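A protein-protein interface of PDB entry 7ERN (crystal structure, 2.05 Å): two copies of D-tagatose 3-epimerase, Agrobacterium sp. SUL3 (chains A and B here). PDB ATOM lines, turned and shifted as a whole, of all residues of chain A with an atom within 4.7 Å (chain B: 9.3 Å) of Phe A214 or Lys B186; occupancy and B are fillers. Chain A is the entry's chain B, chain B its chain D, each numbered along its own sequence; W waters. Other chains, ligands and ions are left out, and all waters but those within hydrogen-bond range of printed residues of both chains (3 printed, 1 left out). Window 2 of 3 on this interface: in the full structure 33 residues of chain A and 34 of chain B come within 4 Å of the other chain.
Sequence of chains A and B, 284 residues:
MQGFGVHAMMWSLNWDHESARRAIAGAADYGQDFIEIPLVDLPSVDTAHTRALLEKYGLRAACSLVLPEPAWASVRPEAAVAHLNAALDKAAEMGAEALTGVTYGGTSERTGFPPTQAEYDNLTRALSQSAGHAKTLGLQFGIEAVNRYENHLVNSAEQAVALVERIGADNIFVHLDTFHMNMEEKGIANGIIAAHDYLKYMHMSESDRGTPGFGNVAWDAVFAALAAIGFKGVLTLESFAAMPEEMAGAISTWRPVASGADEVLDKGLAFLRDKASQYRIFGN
NE of Arg B148 is in salt-bridge range of OE2 of Glu B184, at 2.8 Å.
N of Gly A215 sits close to OE1 of Glu A206, at 3.5 Å.
The backbone carbonyl oxygen (O) of Lys B186 lies within hydrogen-bond range of the side-chain amide nitrogen (ND2) of Asn B190, at 2.7 Å.
The side-chain carboxylate (OD1) of Asp A208 sits at hydrogen-bond distance from the backbone NH (N) of Gly A210, 2.9 Å away.
The side-chain carboxylate (OE1) of Glu A206 is in hydrogen-bond range of the backbone NH (N) of Phe A214 (3.5 Å).
The side-chain carboxylate of Asp A208 lies within salt-bridge range of the side-chain amino group of Lys B186.
The backbone carbonyl oxygen (O) of Val A257 sits at hydrogen-bond distance from the side-chain amino group (NZ) of Lys B186 (2.9 Å).
No residue of chain B comes within 4 Å of Gly A213.
Phe A214 touches just one residue of chain B: Lys B186 (3.3 Å).
Gly A215 touches just one residue of chain B: Gly B187 (3.96 Å).
Printed residues of chain B within 4 Å of Val A257: Lys B186 (2.9 Å).
Lys A267 touches none of the printed residues of chain B.
Printed residues of chain A within 4 Å of Arg B148: Asp A208.
Of chain A, only Asp A208 (2.9 Å), Phe A214 (3.3 Å) and Val A257 (2.9 Å) come within 4 Å of Lys B186.
The nearest residue of chain B that does not touch Phe A214 is Gly B187 (4.8 Å).
The nearest printed residue of chain A that does not touch Lys B186 is Ala A258 (4.6 Å).
The nearest printed residue of chain A that does not touch Met B183 is Glu A206 (6.8 Å).
Water W1 lies within hydrogen-bond range of the side-chain hydroxyl (OG1) of Thr A211 (2.8 Å) and the side-chain amino group (NZ) of Lys B186 (3.0 Å).
Water W3 lies within hydrogen-bond range of O of Phe A214, OD1 of Asp A208, N of Thr A211 and NZ of Lys B186.
Water W2 lies within hydrogen-bond range of the guanidinium group of Arg B148 (2.8 Å) and the backbone carbonyl oxygen of Asp A208 (3.0 Å).
Of the 11 printed residues of chain A, 4 touch a printed residue of chain B.
Of the 19 printed residues of chain B, 4 touch a printed residue of chain A.
Among the printed residues, Asp or Glu carboxylates within 4 Å of a Lys or Arg side-chain nitrogen of the other chain: Asp A208 with Lys B186 (2.9 Å).
No position is printed for both chains.
Of the 6 pairs that touch across the chains among the printed residues, none has its exchanged pair printed and touching as well.
Among the printed residues, pairs that only touch across the chains: Phe A214 with Lys B186, Asp A208 with Met B183, Asp A208 with Arg B148 and Gly A215 with Gly B187.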
ATOM      1  N   GLU A 206      -0.701 -13.272   6.980  1.00  0.00           N
ATOM      2  CA  GLU A 206      -1.305 -14.284   7.832  1.00  0.00           C
ATOM      3  C   GLU A 206      -0.824 -15.681   7.416  1.00  0.00           C
ATOM      4  O   GLU A 206      -0.223 -15.875   6.349  1.00  0.00           O
ATOM      5  CB  GLU A 206      -2.826 -14.170   7.792  1.00  0.00           C
ATOM      6  CG  GLU A 206      -3.539 -14.922   8.893  1.00  0.00           C
ATOM      7  CD  GLU A 206      -2.871 -14.731  10.256  1.00  0.00           C
ATOM      8  OE1 GLU A 206      -3.111 -13.696  10.905  1.00  0.00           O
ATOM      9  OE2 GLU A 206      -2.111 -15.622  10.670  1.00  0.00           O
ATOM     10  N   ASP A 208      -2.332 -18.267   6.418  1.00  0.00           N
ATOM     11  CA  ASP A 208      -2.962 -18.852   5.236  1.00  0.00           C
ATOM     12  C   ASP A 208      -2.944 -17.902   4.044  1.00  0.00           C
ATOM     13  O   ASP A 208      -3.685 -18.128   3.068  1.00  0.00           O
ATOM     14  CB  ASP A 208      -4.399 -19.281   5.543  1.00  0.00           C
ATOM     15  CG  ASP A 208      -5.287 -18.120   5.986  1.00  0.00           C
ATOM     16  OD1 ASP A 208      -4.776 -16.975   6.176  1.00  0.00           O
ATOM     17  OD2 ASP A 208      -6.504 -18.358   6.162  1.00  0.00           O
ATOM     18  N   GLY A 210      -4.147 -15.027   4.098  1.00  0.00           N
ATOM     19  CA  GLY A 210      -5.396 -14.287   4.129  1.00  0.00           C
ATOM     20  C   GLY A 210      -5.301 -12.896   4.739  1.00  0.00           C
ATOM     21  O   GLY A 210      -4.668 -12.003   4.174  1.00  0.00           O
ATOM     22  N   THR A 211      -5.924 -12.705   5.900  1.00  0.00           N
ATOM     23  CA  THR A 211      -6.048 -11.406   6.542  1.00  0.00           C
ATOM     24  C   THR A 211      -5.269 -11.409   7.841  1.00  0.00           C
ATOM     25  O   THR A 211      -5.574 -12.238   8.711  1.00  0.00           O
ATOM     26  CB  THR A 211      -7.523 -11.096   6.815  1.00  0.00           C
ATOM     27  OG1 THR A 211      -8.296 -11.365   5.638  1.00  0.00           O
ATOM     28  CG2 THR A 211      -7.705  -9.635   7.218  1.00  0.00           C
ATOM     29  N   PRO A 212      -4.258 -10.549   8.022  1.00  0.00           N
ATOM     30  CA  PRO A 212      -3.582 -10.478   9.323  1.00  0.00           C
ATOM     31  C   PRO A 212      -4.587 -10.183  10.418  1.00  0.00           C
ATOM     32  O   PRO A 212      -5.475  -9.345  10.251  1.00  0.00           O
ATOM     33  CB  PRO A 212      -2.580  -9.332   9.143  1.00  0.00           C
ATOM     34  CG  PRO A 212      -2.239  -9.418   7.690  1.00  0.00           C
ATOM     35  CD  PRO A 212      -3.560  -9.731   7.015  1.00  0.00           C
ATOM     36  N   GLY A 213      -4.452 -10.906  11.530  1.00  0.00           N
ATOM     37  CA  GLY A 213      -5.427 -10.919  12.587  1.00  0.00           C
ATOM     38  C   GLY A 213      -6.344 -12.126  12.575  1.00  0.00           C
ATOM     39  O   GLY A 213      -6.988 -12.392  13.589  1.00  0.00           O
ATOM     40  N   PHE A 214      -6.416 -12.876  11.460  1.00  0.00           N
ATOM     41  CA  PHE A 214      -7.408 -13.950  11.313  1.00  0.00           C
ATOM     42  C   PHE A 214      -6.736 -15.217  10.803  1.00  0.00           C
ATOM     43  O   PHE A 214      -7.039 -15.734   9.729  1.00  0.00           O
ATOM     44  CB  PHE A 214      -8.568 -13.488  10.417  1.00  0.00           C
ATOM     45  CG  PHE A 214      -9.249 -12.287  10.966  1.00  0.00           C
ATOM     46  CD1 PHE A 214      -8.761 -11.021  10.688  1.00  0.00           C
ATOM     47  CD2 PHE A 214     -10.292 -12.420  11.866  1.00  0.00           C
ATOM     48  CE1 PHE A 214      -9.332  -9.912  11.256  1.00  0.00           C
ATOM     49  CE2 PHE A 214     -10.878 -11.318  12.412  1.00  0.00           C
ATOM     50  CZ  PHE A 214     -10.394 -10.059  12.111  1.00  0.00           C
ATOM     51  N   GLY A 215      -5.822 -15.735  11.619  1.00  0.00           N
ATOM     52  CA  GLY A 215      -5.091 -16.939  11.286  1.00  0.00           C
ATOM     53  C   GLY A 215      -4.285 -17.422  12.469  1.00  0.00           C
ATOM     54  O   GLY A 215      -4.703 -17.264  13.620  1.00  0.00           O
ATOM     55  N   VAL A 257      -8.229 -17.433  -0.264  1.00  0.00           N
ATOM     56  CA  VAL A 257      -7.593 -17.127   1.011  1.00  0.00           C
ATOM     57  C   VAL A 257      -8.424 -16.178   1.860  1.00  0.00           C
ATOM     58  O   VAL A 257      -8.160 -16.062   3.068  1.00  0.00           O
ATOM     59  CB  VAL A 257      -6.185 -16.528   0.814  1.00  0.00           C
ATOM     60  CG1 VAL A 257      -5.247 -17.515   0.120  1.00  0.00           C
ATOM     61  CG2 VAL A 257      -6.281 -15.213   0.036  1.00  0.00           C
ATOM     62  N   ALA A 258      -9.393 -15.486   1.275  1.00  0.00           N
ATOM     63  CA  ALA A 258     -10.192 -14.507   2.017  1.00  0.00           C
ATOM     64  C   ALA A 258     -11.392 -14.122   1.156  1.00  0.00           C
ATOM     65  O   ALA A 258     -11.639 -14.719   0.105  1.00  0.00           O
ATOM     66  CB  ALA A 258      -9.365 -13.281   2.401  1.00  0.00           C
ATOM     67  N   LYS A 267      -9.405  -4.414   6.825  1.00  0.00           N
ATOM     68  CA  LYS A 267      -9.183  -5.056   8.117  1.00  0.00           C
ATOM     69  C   LYS A 267      -7.699  -5.262   8.387  1.00  0.00           C
ATOM     70  O   LYS A 267      -7.221  -5.035   9.510  1.00  0.00           O
ATOM     71  CB  LYS A 267      -9.905  -6.403   8.155  1.00  0.00           C
ATOM     72  CG  LYS A 267     -11.388  -6.353   8.492  1.00  0.00           C
ATOM     73  CD  LYS A 267     -11.856  -7.732   9.009  1.00  0.00           C
ATOM     74  CE  LYS A 267     -11.342  -8.899   8.134  1.00  0.00           C
ATOM     75  NZ  LYS A 267     -11.630 -10.282   8.679  1.00  0.00           N
ATOM     76  N   ARG B 148      -0.832 -27.116   1.134  1.00  0.00           N
ATOM     77  CA  ARG B 148      -0.917 -26.792  -0.288  1.00  0.00           C
ATOM     78  C   ARG B 148       0.351 -27.122  -1.074  1.00  0.00           C
ATOM     79  O   ARG B 148       0.282 -27.280  -2.302  1.00  0.00           O
ATOM     80  CB  ARG B 148      -1.245 -25.308  -0.435  1.00  0.00           C
ATOM     81  CG  ARG B 148      -0.192 -24.395   0.208  1.00  0.00           C
ATOM     82  CD  ARG B 148      -0.749 -23.016   0.526  1.00  0.00           C
ATOM     83  NE  ARG B 148      -1.890 -23.091   1.441  1.00  0.00           N
ATOM     84  CZ  ARG B 148      -2.627 -22.043   1.783  1.00  0.00           C
ATOM     85  NH1 ARG B 148      -2.327 -20.843   1.294  1.00  0.00           N
ATOM     86  NH2 ARG B 148      -3.653 -22.199   2.612  1.00  0.00           N
ATOM     87  N   ASN B 155      -6.504 -30.275   1.495  1.00  0.00           N
ATOM     88  CA  ASN B 155      -5.667 -29.395   2.306  1.00  0.00           C
ATOM     89  C   ASN B 155      -6.331 -28.976   3.608  1.00  0.00           C
ATOM     90  O   ASN B 155      -5.688 -28.978   4.658  1.00  0.00           O
ATOM     91  CB  ASN B 155      -5.295 -28.129   1.529  1.00  0.00           C
ATOM     92  CG  ASN B 155      -4.518 -28.408   0.237  1.00  0.00           C
ATOM     93  OD1 ASN B 155      -4.632 -27.643  -0.714  1.00  0.00           O
ATOM     94  ND2 ASN B 155      -3.712 -29.475   0.208  1.00  0.00           N
ATOM     95  N   SER B 156      -7.601 -28.602   3.559  1.00  0.00           N
ATOM     96  CA  SER B 156      -8.343 -28.161   4.725  1.00  0.00           C
ATOM     97  C   SER B 156      -9.251 -29.277   5.226  1.00  0.00           C
ATOM     98  O   SER B 156      -9.642 -30.171   4.468  1.00  0.00           O
ATOM     99  CB  SER B 156      -9.168 -26.920   4.379  1.00  0.00           C
ATOM    100  OG  SER B 156     -10.278 -27.304   3.565  1.00  0.00           O
ATOM    101  N   ALA B 157      -9.572 -29.221   6.524  1.00  0.00           N
ATOM    102  CA  ALA B 157     -10.535 -30.160   7.096  1.00  0.00           C
ATOM    103  C   ALA B 157     -11.827 -30.191   6.281  1.00  0.00           C
ATOM    104  O   ALA B 157     -12.404 -31.262   6.052  1.00  0.00           O
ATOM    105  CB  ALA B 157     -10.841 -29.781   8.542  1.00  0.00           C
ATOM    106  N   GLU B 158     -12.289 -29.011   5.851  1.00  0.00           N
ATOM    107  CA  GLU B 158     -13.499 -28.875   5.051  1.00  0.00           C
ATOM    108  C   GLU B 158     -13.454 -29.756   3.816  1.00  0.00           C
ATOM    109  O   GLU B 158     -14.432 -30.433   3.478  1.00  0.00           O
ATOM    110  CB  GLU B 158     -13.654 -27.415   4.635  1.00  0.00           C
ATOM    111  CG  GLU B 158     -15.067 -26.989   4.361  1.00  0.00           C
ATOM    112  CD  GLU B 158     -15.360 -25.612   4.940  1.00  0.00           C
ATOM    113  OE1 GLU B 158     -15.325 -24.616   4.176  1.00  0.00           O
ATOM    114  OE2 GLU B 158     -15.614 -25.532   6.164  1.00  0.00           O
ATOM    115  N   HIS B 180       0.222 -29.220   9.316  1.00  0.00           N
ATOM    116  CA  HIS B 180      -0.385 -28.766   8.066  1.00  0.00           C
ATOM    117  C   HIS B 180      -1.499 -27.761   8.327  1.00  0.00           C
ATOM    118  O   HIS B 180      -1.658 -26.787   7.576  1.00  0.00           O
ATOM    119  CB  HIS B 180      -0.917 -29.969   7.290  1.00  0.00           C
ATOM    120  CG  HIS B 180       0.156 -30.902   6.822  1.00  0.00           C
ATOM    121  ND1 HIS B 180       1.148 -30.516   5.945  1.00  0.00           N
ATOM    122  CD2 HIS B 180       0.386 -32.207   7.098  1.00  0.00           C
ATOM    123  CE1 HIS B 180       1.937 -31.546   5.698  1.00  0.00           C
ATOM    124  NE2 HIS B 180       1.498 -32.583   6.390  1.00  0.00           N
ATOM    125  N   MET B 181      -2.257 -27.977   9.405  1.00  0.00           N
ATOM    126  CA  MET B 181      -3.317 -27.051   9.788  1.00  0.00           C
ATOM    127  C   MET B 181      -2.779 -25.672  10.123  1.00  0.00           C
ATOM    128  O   MET B 181      -3.466 -24.672   9.899  1.00  0.00           O
ATOM    129  CB  MET B 181      -4.070 -27.601  10.989  1.00  0.00           C
ATOM    130  CG  MET B 181      -5.011 -28.755  10.661  1.00  0.00           C
ATOM    131  SD  MET B 181      -6.076 -29.042  12.098  1.00  0.00           S
ATOM    132  CE  MET B 181      -4.954 -29.985  13.036  1.00  0.00           C
ATOM    133  N   ASN B 182      -1.581 -25.607  10.714  1.00  0.00           N
ATOM    134  CA  ASN B 182      -0.994 -24.324  11.077  1.00  0.00           C
ATOM    135  C   ASN B 182      -0.905 -23.407   9.862  1.00  0.00           C
ATOM    136  O   ASN B 182      -0.960 -22.176  10.001  1.00  0.00           O
ATOM    137  CB  ASN B 182       0.375 -24.568  11.709  1.00  0.00           C
ATOM    138  CG  ASN B 182       0.924 -23.341  12.400  1.00  0.00           C
ATOM    139  OD1 ASN B 182       0.218 -22.677  13.147  1.00  0.00           O
ATOM    140  ND2 ASN B 182       2.192 -23.034  12.138  1.00  0.00           N
ATOM    141  N   MET B 183      -0.839 -23.988   8.659  1.00  0.00           N
ATOM    142  CA  MET B 183      -0.908 -23.234   7.408  1.00  0.00           C
ATOM    143  C   MET B 183      -2.321 -23.206   6.823  1.00  0.00           C
ATOM    144  O   MET B 183      -2.809 -22.144   6.414  1.00  0.00           O
ATOM    145  CB  MET B 183       0.066 -23.827   6.378  1.00  0.00           C
ATOM    146  CG  MET B 183      -0.008 -23.138   5.003  1.00  0.00           C
ATOM    147  SD  MET B 183       1.209 -23.761   3.804  1.00  0.00           S
ATOM    148  CE  MET B 183       2.749 -23.227   4.565  1.00  0.00           C
ATOM    149  N   GLU B 184      -3.005 -24.356   6.802  1.00  0.00           N
ATOM    150  CA  GLU B 184      -4.223 -24.482   6.001  1.00  0.00           C
ATOM    151  C   GLU B 184      -5.483 -23.967   6.693  1.00  0.00           C
ATOM    152  O   GLU B 184      -6.419 -23.552   6.001  1.00  0.00           O
ATOM    153  CB  GLU B 184      -4.426 -25.936   5.596  1.00  0.00           C
ATOM    154  CG  GLU B 184      -3.362 -26.458   4.624  1.00  0.00           C
ATOM    155  CD  GLU B 184      -3.200 -25.582   3.388  1.00  0.00           C
ATOM    156  OE1 GLU B 184      -4.220 -25.088   2.843  1.00  0.00           O
ATOM    157  OE2 GLU B 184      -2.042 -25.393   2.962  1.00  0.00           O
ATOM    158  N   GLU B 185      -5.558 -23.981   8.026  1.00  0.00           N
ATOM    159  CA  GLU B 185      -6.802 -23.606   8.690  1.00  0.00           C
ATOM    160  C   GLU B 185      -6.766 -22.145   9.119  1.00  0.00           C
ATOM    161  O   GLU B 185      -5.737 -21.634   9.580  1.00  0.00           O
ATOM    162  CB  GLU B 185      -7.110 -24.513   9.887  1.00  0.00           C
ATOM    163  CG  GLU B 185      -6.996 -26.016   9.580  1.00  0.00           C
ATOM    164  CD  GLU B 185      -8.095 -26.574   8.645  1.00  0.00           C
ATOM    165  OE1 GLU B 185      -9.140 -25.911   8.465  1.00  0.00           O
ATOM    166  OE2 GLU B 185      -7.915 -27.705   8.111  1.00  0.00           O
ATOM    167  N   LYS B 186      -7.895 -21.463   8.905  1.00  0.00           N
ATOM    168  CA  LYS B 186      -8.063 -20.056   9.273  1.00  0.00           C
ATOM    169  C   LYS B 186      -8.413 -20.030  10.760  1.00  0.00           C
ATOM    170  O   LYS B 186      -9.567 -19.891  11.173  1.00  0.00           O
ATOM    171  CB  LYS B 186      -9.127 -19.393   8.400  1.00  0.00           C
ATOM    172  CG  LYS B 186      -9.195 -17.868   8.494  1.00  0.00           C
ATOM    173  CD  LYS B 186     -10.371 -17.304   7.684  1.00  0.00           C
ATOM    174  CE  LYS B 186     -10.156 -17.482   6.186  1.00  0.00           C
ATOM    175  NZ  LYS B 186      -8.897 -16.793   5.734  1.00  0.00           N
ATOM    176  N   GLY B 187      -7.376 -20.155  11.582  1.00  0.00           N
ATOM    177  CA  GLY B 187      -7.565 -20.489  12.975  1.00  0.00           C
ATOM    178  C   GLY B 187      -7.538 -21.997  13.065  1.00  0.00           C
ATOM    179  O   GLY B 187      -8.446 -22.678  12.569  1.00  0.00           O
ATOM    180  N   ILE B 188      -6.476 -22.530  13.673  1.00  0.00           N
ATOM    181  CA  ILE B 188      -6.223 -23.969  13.631  1.00  0.00           C
ATOM    182  C   ILE B 188      -7.414 -24.750  14.185  1.00  0.00           C
ATOM    183  O   ILE B 188      -7.778 -25.815  13.658  1.00  0.00           O
ATOM    184  CB  ILE B 188      -4.910 -24.284  14.375  1.00  0.00           C
ATOM    185  CG1 ILE B 188      -4.502 -25.740  14.179  1.00  0.00           C
ATOM    186  CG2 ILE B 188      -5.009 -23.931  15.886  1.00  0.00           C
ATOM    187  CD1 ILE B 188      -3.004 -25.973  14.413  1.00  0.00           C
ATOM    188  N   ALA B 189      -8.074 -24.218  15.227  1.00  0.00           N
ATOM    189  CA  ALA B 189      -9.192 -24.936  15.829  1.00  0.00           C
ATOM    190  C   ALA B 189     -10.372 -25.079  14.882  1.00  0.00           C
ATOM    191  O   ALA B 189     -11.195 -25.988  15.071  1.00  0.00           O
ATOM    192  CB  ALA B 189      -9.659 -24.247  17.107  1.00  0.00           C
ATOM    193  N   ASN B 190     -10.477 -24.206  13.874  1.00  0.00           N
ATOM    194  CA  ASN B 190     -11.560 -24.309  12.896  1.00  0.00           C
ATOM    195  C   ASN B 190     -11.504 -25.607  12.099  1.00  0.00           C
ATOM    196  O   ASN B 190     -12.542 -26.094  11.632  1.00  0.00           O
ATOM    197  CB  ASN B 190     -11.516 -23.122  11.943  1.00  0.00           C
ATOM    198  CG  ASN B 190     -12.392 -21.997  12.411  1.00  0.00           C
ATOM    199  OD1 ASN B 190     -13.453 -22.242  12.984  1.00  0.00           O
ATOM    200  ND2 ASN B 190     -11.950 -20.754  12.201  1.00  0.00           N
ATOM    201  N   GLY B 191     -10.312 -26.161  11.895  1.00  0.00           N
ATOM    202  CA  GLY B 191     -10.226 -27.416  11.167  1.00  0.00           C
ATOM    203  C   GLY B 191     -10.759 -28.566  11.992  1.00  0.00           C
ATOM    204  O   GLY B 191     -11.499 -29.425  11.485  1.00  0.00           O
ATOM    205  N   ILE B 192     -10.420 -28.580  13.284  1.00  0.00           N
ATOM    206  CA  ILE B 192     -10.932 -29.611  14.177  1.00  0.00           C
ATOM    207  C   ILE B 192     -12.448 -29.506  14.271  1.00  0.00           C
ATOM    208  O   ILE B 192     -13.160 -30.511  14.201  1.00  0.00           O
ATOM    209  CB  ILE B 192     -10.247 -29.509  15.559  1.00  0.00           C
ATOM    210  CG1 ILE B 192      -8.797 -30.017  15.469  1.00  0.00           C
ATOM    211  CG2 ILE B 192     -11.039 -30.280  16.647  1.00  0.00           C
ATOM    212  CD1 ILE B 192      -7.875 -29.404  16.538  1.00  0.00           C
ATOM    213  N   ILE B 193     -12.967 -28.286  14.371  1.00  0.00           N
ATOM    214  CA  ILE B 193     -14.406 -28.109  14.509  1.00  0.00           C
ATOM    215  C   ILE B 193     -15.133 -28.580  13.254  1.00  0.00           C
ATOM    216  O   ILE B 193     -16.143 -29.287  13.337  1.00  0.00           O
ATOM    217  CB  ILE B 193     -14.728 -26.643  14.840  1.00  0.00           C
ATOM    218  CG1 ILE B 193     -14.217 -26.327  16.252  1.00  0.00           C
ATOM    219  CG2 ILE B 193     -16.215 -26.414  14.761  1.00  0.00           C
ATOM    220  CD1 ILE B 193     -14.065 -24.840  16.557  1.00  0.00           C
HETATM  221  O   HOH W   1      -9.502 -13.836   5.860  1.00  0.00           O
HETATM  222  O   HOH W   2      -5.713 -20.264   2.550  1.00  0.00           O
HETATM  223  O   HOH W   3      -6.728 -15.164   7.027  1.00  0.00           O
